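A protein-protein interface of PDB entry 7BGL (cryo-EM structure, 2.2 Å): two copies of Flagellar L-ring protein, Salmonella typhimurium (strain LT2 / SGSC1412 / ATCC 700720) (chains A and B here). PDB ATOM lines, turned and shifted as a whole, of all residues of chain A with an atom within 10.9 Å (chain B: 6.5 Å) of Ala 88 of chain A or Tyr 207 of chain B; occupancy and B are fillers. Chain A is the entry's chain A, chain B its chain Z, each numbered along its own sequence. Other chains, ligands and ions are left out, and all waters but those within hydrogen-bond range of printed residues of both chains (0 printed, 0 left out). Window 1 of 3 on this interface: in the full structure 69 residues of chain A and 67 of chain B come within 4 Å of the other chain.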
ATOM      1  N   GLU A  84      15.888  18.652  26.790  1.00  0.00           N
ATOM      2  CA  GLU A  84      14.724  19.417  26.370  1.00  0.00           C
ATOM      3  C   GLU A  84      13.942  18.635  25.327  1.00  0.00           C
ATOM      4  O   GLU A  84      14.524  18.044  24.417  1.00  0.00           O
ATOM      5  CB  GLU A  84      15.144  20.773  25.802  1.00  0.00           C
ATOM      6  CG  GLU A  84      15.545  21.787  26.857  1.00  0.00           C
ATOM      7  CD  GLU A  84      14.362  22.516  27.453  1.00  0.00           C
ATOM      8  OE1 GLU A  84      13.299  21.887  27.637  1.00  0.00           O
ATOM      9  OE2 GLU A  84      14.494  23.723  27.752  1.00  0.00           O
ATOM     10  N   ASN A  85      12.619  18.639  25.461  1.00  0.00           N
ATOM     11  CA  ASN A  85      11.758  17.899  24.542  1.00  0.00           C
ATOM     12  C   ASN A  85      10.391  18.563  24.536  1.00  0.00           C
ATOM     13  O   ASN A  85       9.651  18.467  25.520  1.00  0.00           O
ATOM     14  CB  ASN A  85      11.654  16.433  24.951  1.00  0.00           C
ATOM     15  CG  ASN A  85      10.970  15.583  23.903  1.00  0.00           C
ATOM     16  OD1 ASN A  85      10.217  16.088  23.071  1.00  0.00           O
ATOM     17  ND2 ASN A  85      11.229  14.284  23.938  1.00  0.00           N
ATOM     18  N   VAL A  86      10.053  19.229  23.435  1.00  0.00           N
ATOM     19  CA  VAL A  86       8.767  19.900  23.287  1.00  0.00           C
ATOM     20  C   VAL A  86       8.102  19.395  22.018  1.00  0.00           C
ATOM     21  O   VAL A  86       8.766  19.200  20.994  1.00  0.00           O
ATOM     22  CB  VAL A  86       8.920  21.434  23.250  1.00  0.00           C
ATOM     23  CG1 VAL A  86       7.576  22.092  22.996  1.00  0.00           C
ATOM     24  CG2 VAL A  86       9.528  21.935  24.548  1.00  0.00           C
ATOM     25  N   SER A  87       6.793  19.168  22.091  1.00  0.00           N
ATOM     26  CA  SER A  87       6.032  18.699  20.942  1.00  0.00           C
ATOM     27  C   SER A  87       4.611  19.230  21.037  1.00  0.00           C
ATOM     28  O   SER A  87       3.932  19.010  22.043  1.00  0.00           O
ATOM     29  CB  SER A  87       6.024  17.169  20.871  1.00  0.00           C
ATOM     30  OG  SER A  87       5.085  16.708  19.917  1.00  0.00           O
ATOM     31  N   ALA A  88       4.170  19.926  19.993  1.00  0.00           N
ATOM     32  CA  ALA A  88       2.830  20.488  19.929  1.00  0.00           C
ATOM     33  C   ALA A  88       2.211  20.162  18.580  1.00  0.00           C
ATOM     34  O   ALA A  88       2.884  20.218  17.545  1.00  0.00           O
ATOM     35  CB  ALA A  88       2.849  22.004  20.145  1.00  0.00           C
ATOM     36  N   SER A  89       0.925  19.816  18.598  1.00  0.00           N
ATOM     37  CA  SER A  89       0.197  19.456  17.393  1.00  0.00           C
ATOM     38  C   SER A  89      -1.169  20.123  17.410  1.00  0.00           C
ATOM     39  O   SER A  89      -1.721  20.424  18.471  1.00  0.00           O
ATOM     40  CB  SER A  89       0.036  17.936  17.262  1.00  0.00           C
ATOM     41  OG  SER A  89      -0.107  17.556  15.906  1.00  0.00           O
ATOM     42  N   LYS A  90      -1.710  20.346  16.215  1.00  0.00           N
ATOM     43  CA  LYS A  90      -2.986  21.025  16.048  1.00  0.00           C
ATOM     44  C   LYS A  90      -3.628  20.533  14.762  1.00  0.00           C
ATOM     45  O   LYS A  90      -2.956  20.453  13.731  1.00  0.00           O
ATOM     46  CB  LYS A  90      -2.790  22.542  16.008  1.00  0.00           C
ATOM     47  CG  LYS A  90      -3.881  23.300  15.285  1.00  0.00           C
ATOM     48  CD  LYS A  90      -3.641  24.798  15.361  1.00  0.00           C
ATOM     49  CE  LYS A  90      -2.429  25.213  14.551  1.00  0.00           C
ATOM     50  NZ  LYS A  90      -2.263  26.691  14.557  1.00  0.00           N
ATOM     51  N   SER A  91      -4.915  20.205  14.825  1.00  0.00           N
ATOM     52  CA  SER A  91      -5.641  19.723  13.660  1.00  0.00           C
ATOM     53  C   SER A  91      -7.066  20.251  13.692  1.00  0.00           C
ATOM     54  O   SER A  91      -7.619  20.528  14.759  1.00  0.00           O
ATOM     55  CB  SER A  91      -5.654  18.192  13.594  1.00  0.00           C
ATOM     56  OG  SER A  91      -4.414  17.694  13.125  1.00  0.00           O
ATOM     57  N   GLY A 137      -3.898  21.960   9.678  1.00  0.00           N
ATOM     58  CA  GLY A 137      -3.053  21.287  10.647  1.00  0.00           C
ATOM     59  C   GLY A 137      -1.766  22.048  10.860  1.00  0.00           C
ATOM     60  O   GLY A 137      -1.418  22.959  10.108  1.00  0.00           O
ATOM     61  N   ALA A 138      -1.060  21.651  11.914  1.00  0.00           N
ATOM     62  CA  ALA A 138       0.193  22.295  12.280  1.00  0.00           C
ATOM     63  C   ALA A 138       0.908  21.438  13.310  1.00  0.00           C
ATOM     64  O   ALA A 138       0.264  20.812  14.155  1.00  0.00           O
ATOM     65  CB  ALA A 138      -0.052  23.705  12.832  1.00  0.00           C
ATOM     66  N   ASN A 139       2.234  21.403  13.225  1.00  0.00           N
ATOM     67  CA  ASN A 139       3.059  20.657  14.161  1.00  0.00           C
ATOM     68  C   ASN A 139       4.320  21.449  14.467  1.00  0.00           C
ATOM     69  O   ASN A 139       4.772  22.262  13.657  1.00  0.00           O
ATOM     70  CB  ASN A 139       3.435  19.276  13.611  1.00  0.00           C
ATOM     71  CG  ASN A 139       2.230  18.486  13.145  1.00  0.00           C
ATOM     72  OD1 ASN A 139       1.715  17.636  13.871  1.00  0.00           O
ATOM     73  ND2 ASN A 139       1.775  18.763  11.930  1.00  0.00           N
ATOM     74  N   ALA A 140       4.882  21.207  15.648  1.00  0.00           N
ATOM     75  CA  ALA A 140       6.133  21.856  16.033  1.00  0.00           C
ATOM     76  C   ALA A 140       6.779  21.040  17.137  1.00  0.00           C
ATOM     77  O   ALA A 140       6.214  20.922  18.226  1.00  0.00           O
ATOM     78  CB  ALA A 140       5.887  23.292  16.490  1.00  0.00           C
ATOM     79  N   SER A 141       7.955  20.484  16.865  1.00  0.00           N
ATOM     80  CA  SER A 141       8.665  19.682  17.848  1.00  0.00           C
ATOM     81  C   SER A 141      10.133  20.079  17.866  1.00  0.00           C
ATOM     82  O   SER A 141      10.681  20.542  16.862  1.00  0.00           O
ATOM     83  CB  SER A 141       8.528  18.181  17.560  1.00  0.00           C
ATOM     84  OG  SER A 141       9.349  17.793  16.474  1.00  0.00           O
ATOM     85  N   ASN A 142      10.761  19.895  19.023  1.00  0.00           N
ATOM     86  CA  ASN A 142      12.182  20.164  19.173  1.00  0.00           C
ATOM     87  C   ASN A 142      12.734  19.313  20.306  1.00  0.00           C
ATOM     88  O   ASN A 142      12.030  19.007  21.274  1.00  0.00           O
ATOM     89  CB  ASN A 142      12.455  21.650  19.437  1.00  0.00           C
ATOM     90  CG  ASN A 142      11.964  22.098  20.795  1.00  0.00           C
ATOM     91  OD1 ASN A 142      10.776  22.012  21.098  1.00  0.00           O
ATOM     92  ND2 ASN A 142      12.880  22.580  21.623  1.00  0.00           N
ATOM     93  N   THR A 143      14.003  18.933  20.168  1.00  0.00           N
ATOM     94  CA  THR A 143      14.685  18.103  21.149  1.00  0.00           C
ATOM     95  C   THR A 143      16.115  18.590  21.323  1.00  0.00           C
ATOM     96  O   THR A 143      16.704  19.183  20.415  1.00  0.00           O
ATOM     97  CB  THR A 143      14.687  16.623  20.741  1.00  0.00           C
ATOM     98  OG1 THR A 143      15.417  16.462  19.520  1.00  0.00           O
ATOM     99  CG2 THR A 143      13.266  16.124  20.544  1.00  0.00           C
ATOM    100  N   PHE A 144      16.664  18.332  22.507  1.00  0.00           N
ATOM    101  CA  PHE A 144      18.019  18.735  22.858  1.00  0.00           C
ATOM    102  C   PHE A 144      18.527  17.779  23.927  1.00  0.00           C
ATOM    103  O   PHE A 144      17.878  17.621  24.964  1.00  0.00           O
ATOM    104  CB  PHE A 144      18.050  20.178  23.369  1.00  0.00           C
ATOM    105  CG  PHE A 144      19.205  20.981  22.849  1.00  0.00           C
ATOM    106  CD1 PHE A 144      20.507  20.572  23.073  1.00  0.00           C
ATOM    107  CD2 PHE A 144      18.989  22.152  22.146  1.00  0.00           C
ATOM    108  CE1 PHE A 144      21.570  21.311  22.600  1.00  0.00           C
ATOM    109  CE2 PHE A 144      20.048  22.896  21.671  1.00  0.00           C
ATOM    110  CZ  PHE A 144      21.341  22.475  21.899  1.00  0.00           C
ATOM    111  N   THR B 143      -2.604  19.284  20.878  1.00  0.00           N
ATOM    112  CA  THR B 143      -1.807  18.618  21.897  1.00  0.00           C
ATOM    113  C   THR B 143      -0.541  19.421  22.158  1.00  0.00           C
ATOM    114  O   THR B 143      -0.053  20.147  21.289  1.00  0.00           O
ATOM    115  CB  THR B 143      -1.438  17.186  21.488  1.00  0.00           C
ATOM    116  OG1 THR B 143      -0.620  17.217  20.313  1.00  0.00           O
ATOM    117  CG2 THR B 143      -2.690  16.375  21.204  1.00  0.00           C
ATOM    118  N   PHE B 144      -0.017  19.277  23.373  1.00  0.00           N
ATOM    119  CA  PHE B 144       1.185  19.976  23.806  1.00  0.00           C
ATOM    120  C   PHE B 144       1.837  19.149  24.901  1.00  0.00           C
ATOM    121  O   PHE B 144       1.182  18.828  25.896  1.00  0.00           O
ATOM    122  CB  PHE B 144       0.851  21.380  24.320  1.00  0.00           C
ATOM    123  CG  PHE B 144       1.815  22.437  23.873  1.00  0.00           C
ATOM    124  CD1 PHE B 144       3.161  22.337  24.174  1.00  0.00           C
ATOM    125  CD2 PHE B 144       1.374  23.537  23.161  1.00  0.00           C
ATOM    126  CE1 PHE B 144       4.049  23.310  23.768  1.00  0.00           C
ATOM    127  CE2 PHE B 144       2.257  24.514  22.753  1.00  0.00           C
ATOM    128  CZ  PHE B 144       3.597  24.401  23.057  1.00  0.00           C
ATOM    129  N   SER B 145       3.112  18.812  24.726  1.00  0.00           N
ATOM    130  CA  SER B 145       3.797  17.853  25.590  1.00  0.00           C
ATOM    131  C   SER B 145       5.168  18.371  26.008  1.00  0.00           C
ATOM    132  O   SER B 145       6.179  17.673  25.907  1.00  0.00           O
ATOM    133  CB  SER B 145       3.923  16.500  24.898  1.00  0.00           C
ATOM    134  OG  SER B 145       4.818  15.653  25.597  1.00  0.00           O
ATOM    135  N   GLU B 176      13.280  29.251  18.052  1.00  0.00           N
ATOM    136  CA  GLU B 176      11.957  28.899  18.543  1.00  0.00           C
ATOM    137  C   GLU B 176      11.733  29.572  19.886  1.00  0.00           C
ATOM    138  O   GLU B 176      12.598  29.508  20.767  1.00  0.00           O
ATOM    139  CB  GLU B 176      11.795  27.387  18.693  1.00  0.00           C
ATOM    140  CG  GLU B 176      11.721  26.619  17.390  1.00  0.00           C
ATOM    141  CD  GLU B 176      11.785  25.120  17.622  1.00  0.00           C
ATOM    142  OE1 GLU B 176      10.957  24.597  18.394  1.00  0.00           O
ATOM    143  OE2 GLU B 176      12.674  24.464  17.048  1.00  0.00           O
ATOM    144  N   PHE B 177      10.577  30.205  20.042  1.00  0.00           N
ATOM    145  CA  PHE B 177      10.176  30.824  21.298  1.00  0.00           C
ATOM    146  C   PHE B 177       8.985  30.063  21.861  1.00  0.00           C
ATOM    147  O   PHE B 177       7.964  29.911  21.182  1.00  0.00           O
ATOM    148  CB  PHE B 177       9.819  32.298  21.099  1.00  0.00           C
ATOM    149  CG  PHE B 177      10.846  33.075  20.330  1.00  0.00           C
ATOM    150  CD1 PHE B 177      10.846  33.069  18.947  1.00  0.00           C
ATOM    151  CD2 PHE B 177      11.806  33.819  20.992  1.00  0.00           C
ATOM    152  CE1 PHE B 177      11.788  33.784  18.240  1.00  0.00           C
ATOM    153  CE2 PHE B 177      12.751  34.536  20.288  1.00  0.00           C
ATOM    154  CZ  PHE B 177      12.741  34.518  18.910  1.00  0.00           C
ATOM    155  N   ILE B 178       9.118  29.587  23.095  1.00  0.00           N
ATOM    156  CA  ILE B 178       8.035  28.947  23.828  1.00  0.00           C
ATOM    157  C   ILE B 178       7.752  29.827  25.033  1.00  0.00           C
ATOM    158  O   ILE B 178       8.594  29.946  25.931  1.00  0.00           O
ATOM    159  CB  ILE B 178       8.391  27.520  24.262  1.00  0.00           C
ATOM    160  CG1 ILE B 178       8.841  26.691  23.059  1.00  0.00           C
ATOM    161  CG2 ILE B 178       7.210  26.861  24.959  1.00  0.00           C
ATOM    162  CD1 ILE B 178       9.143  25.252  23.394  1.00  0.00           C
ATOM    163  N   ARG B 179       6.581  30.450  25.056  1.00  0.00           N
ATOM    164  CA  ARG B 179       6.208  31.351  26.135  1.00  0.00           C
ATOM    165  C   ARG B 179       4.900  30.901  26.764  1.00  0.00           C
ATOM    166  O   ARG B 179       3.988  30.435  26.073  1.00  0.00           O
ATOM    167  CB  ARG B 179       6.088  32.796  25.643  1.00  0.00           C
ATOM    168  CG  ARG B 179       5.737  32.935  24.180  1.00  0.00           C
ATOM    169  CD  ARG B 179       5.663  34.399  23.787  1.00  0.00           C
ATOM    170  NE  ARG B 179       6.986  34.993  23.640  1.00  0.00           N
ATOM    171  CZ  ARG B 179       7.567  35.240  22.474  1.00  0.00           C
ATOM    172  NH1 ARG B 179       6.969  34.956  21.330  1.00  0.00           N
ATOM    173  NH2 ARG B 179       8.778  35.789  22.457  1.00  0.00           N
ATOM    174  N   ILE B 205      -0.359  30.029  25.837  1.00  0.00           N
ATOM    175  CA  ILE B 205       0.771  29.217  25.402  1.00  0.00           C
ATOM    176  C   ILE B 205       1.096  29.597  23.967  1.00  0.00           C
ATOM    177  O   ILE B 205       0.217  29.558  23.095  1.00  0.00           O
ATOM    178  CB  ILE B 205       0.474  27.715  25.521  1.00  0.00           C
ATOM    179  CG1 ILE B 205      -0.141  27.398  26.885  1.00  0.00           C
ATOM    180  CG2 ILE B 205       1.739  26.904  25.307  1.00  0.00           C
ATOM    181  CD1 ILE B 205      -0.766  26.026  26.967  1.00  0.00           C
ATOM    182  N   GLU B 206       2.349  29.967  23.722  1.00  0.00           N
ATOM    183  CA  GLU B 206       2.834  30.288  22.388  1.00  0.00           C
ATOM    184  C   GLU B 206       4.067  29.452  22.092  1.00  0.00           C
ATOM    185  O   GLU B 206       4.948  29.315  22.946  1.00  0.00           O
ATOM    186  CB  GLU B 206       3.172  31.774  22.254  1.00  0.00           C
ATOM    187  CG  GLU B 206       3.202  32.260  20.816  1.00  0.00           C
ATOM    188  CD  GLU B 206       3.417  33.753  20.706  1.00  0.00           C
ATOM    189  OE1 GLU B 206       3.702  34.391  21.740  1.00  0.00           O
ATOM    190  OE2 GLU B 206       3.307  34.290  19.584  1.00  0.00           O
ATOM    191  N   TYR B 207       4.124  28.899  20.882  1.00  0.00           N
ATOM    192  CA  TYR B 207       5.269  28.119  20.409  1.00  0.00           C
ATOM    193  C   TYR B 207       5.519  28.556  18.967  1.00  0.00           C
ATOM    194  O   TYR B 207       5.007  27.951  18.026  1.00  0.00           O
ATOM    195  CB  TYR B 207       4.994  26.624  20.520  1.00  0.00           C
ATOM    196  CG  TYR B 207       6.157  25.735  20.151  1.00  0.00           C
ATOM    197  CD1 TYR B 207       7.418  26.264  19.922  1.00  0.00           C
ATOM    198  CD2 TYR B 207       5.993  24.362  20.038  1.00  0.00           C
ATOM    199  CE1 TYR B 207       8.479  25.454  19.588  1.00  0.00           C
ATOM    200  CE2 TYR B 207       7.050  23.543  19.705  1.00  0.00           C
ATOM    201  CZ  TYR B 207       8.291  24.095  19.481  1.00  0.00           C
ATOM    202  OH  TYR B 207       9.351  23.285  19.147  1.00  0.00           O
ATOM    203  N   VAL B 208       6.326  29.601  18.798  1.00  0.00           N
ATOM    204  CA  VAL B 208       6.511  30.229  17.498  1.00  0.00           C
ATOM    205  C   VAL B 208       7.944  30.007  17.034  1.00  0.00           C
ATOM    206  O   VAL B 208       8.829  29.656  17.814  1.00  0.00           O
ATOM    207  CB  VAL B 208       6.171  31.732  17.522  1.00  0.00           C
ATOM    208  CG1 VAL B 208       4.674  31.930  17.674  1.00  0.00           C
ATOM    209  CG2 VAL B 208       6.923  32.429  18.640  1.00  0.00           C
ATOM    210  N   GLY B 209       8.164  30.221  15.732  1.00  0.00           N
ATOM    211  CA  GLY B 209       9.471  30.024  15.146  1.00  0.00           C
ATOM    212  C   GLY B 209       9.846  31.172  14.228  1.00  0.00           C
ATOM    213  O   GLY B 209       9.012  32.000  13.854  1.00  0.00           O
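Among the printed residues, pairs that only touch across the chains: Asn 85 of chain A with Ser 145 of chain B (3.6 Å), Val 86 of chain A with Phe 144 of chain B (3.8 Å), Val 86 of chain A with Ile 178 of chain B (3.5 Å), Val 86 of chain A with Tyr 207 of chain B (3.6 Å), Ser 87 of chain A with Phe 144 of chain B (3.4 Å), Ala 88 of chain A with Thr 143 of chain B (3.2 Å), Ala 88 of chain A with Phe 144 of chain B (3.7 Å), Ala 88 of chain A with Tyr 207 of chain B (3.9 Å), Ala 140 of chain A with Tyr 207 of chain B (3.1 Å), Ser 141 of chain A with Tyr 207 of chain B (3.5 Å) and Asn 142 of chain A with Glu 176 of chain B (3.5 Å).
2 positions are printed for both chains.
Of the 14 pairs that touch across the chains among the printed residues, none has its exchanged pair printed and touching as well.
Of the 12 printed residues of chain B, 6 touch a printed residue of chain A.
Printed residues of chain B that touch a printed residue of chain A: Thr 143, Phe 144, Ser 145, Glu 176, Ile 178 and Tyr 207.
Hydrophobic or aromatic side chains of chain B that line the printed part of chain A: Phe 144, Ile 178 and Tyr 207.
Among the printed residues, 14 pairs touch across the chains.
N of Ala 88 of chain A is in hydrogen-bond range of O of Ala 140 of chain A (2.9 Å).
The side-chain hydroxyl (OG) of Ser 89 of chain A is in hydrogen-bond range of the side-chain amide oxygen (OD1) of Asn 139 of chain A (2.7 Å).
The backbone carbonyl oxygen of Val 86 of chain A is in hydrogen-bond range of the backbone NH of Asn 142 of chain A (2.9 Å).
O of Ser 87 of chain A lies within hydrogen-bond range of N of Ser 145 of chain B (2.8 Å).
N of Thr 143 of chain B is in hydrogen-bond range of O of Ser 89 of chain A (2.8 Å).
The side-chain amide oxygen (OD1) of Asn 142 of chain A is in hydrogen-bond range of the side-chain hydroxyl (OH) of Tyr 207 of chain B (2.7 Å).
Of the printed residues of chain B, Asn 85 of chain A touches Ser 145 (3.6 Å).
Of chain B, only Thr 143, Phe 144 and Tyr 207 come within 4 Å of Ala 88 of chain A.
Printed residues of chain B within 4 Å of Ser 89 of chain A: Thr 143.
Of the printed residues of chain B, Ser 141 of chain A touches Tyr 207 (3.5 Å).
Thr 143 of chain B touches two residues of chain A.
Ile 178 of chain B touches one residue of chain A.
No residue of chain A comes within 4 Å of Glu 206 of chain B.
No residue of chain A comes within 4 Å of Val 208 of chain B.
The nearest residue of chain B that does not touch Ala 88 of chain A is Ser 145 of chain B (5.0 Å).
The nearest printed residue of chain B that does not touch Val 86 of chain A is Ser 145 of chain B (4.3 Å).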
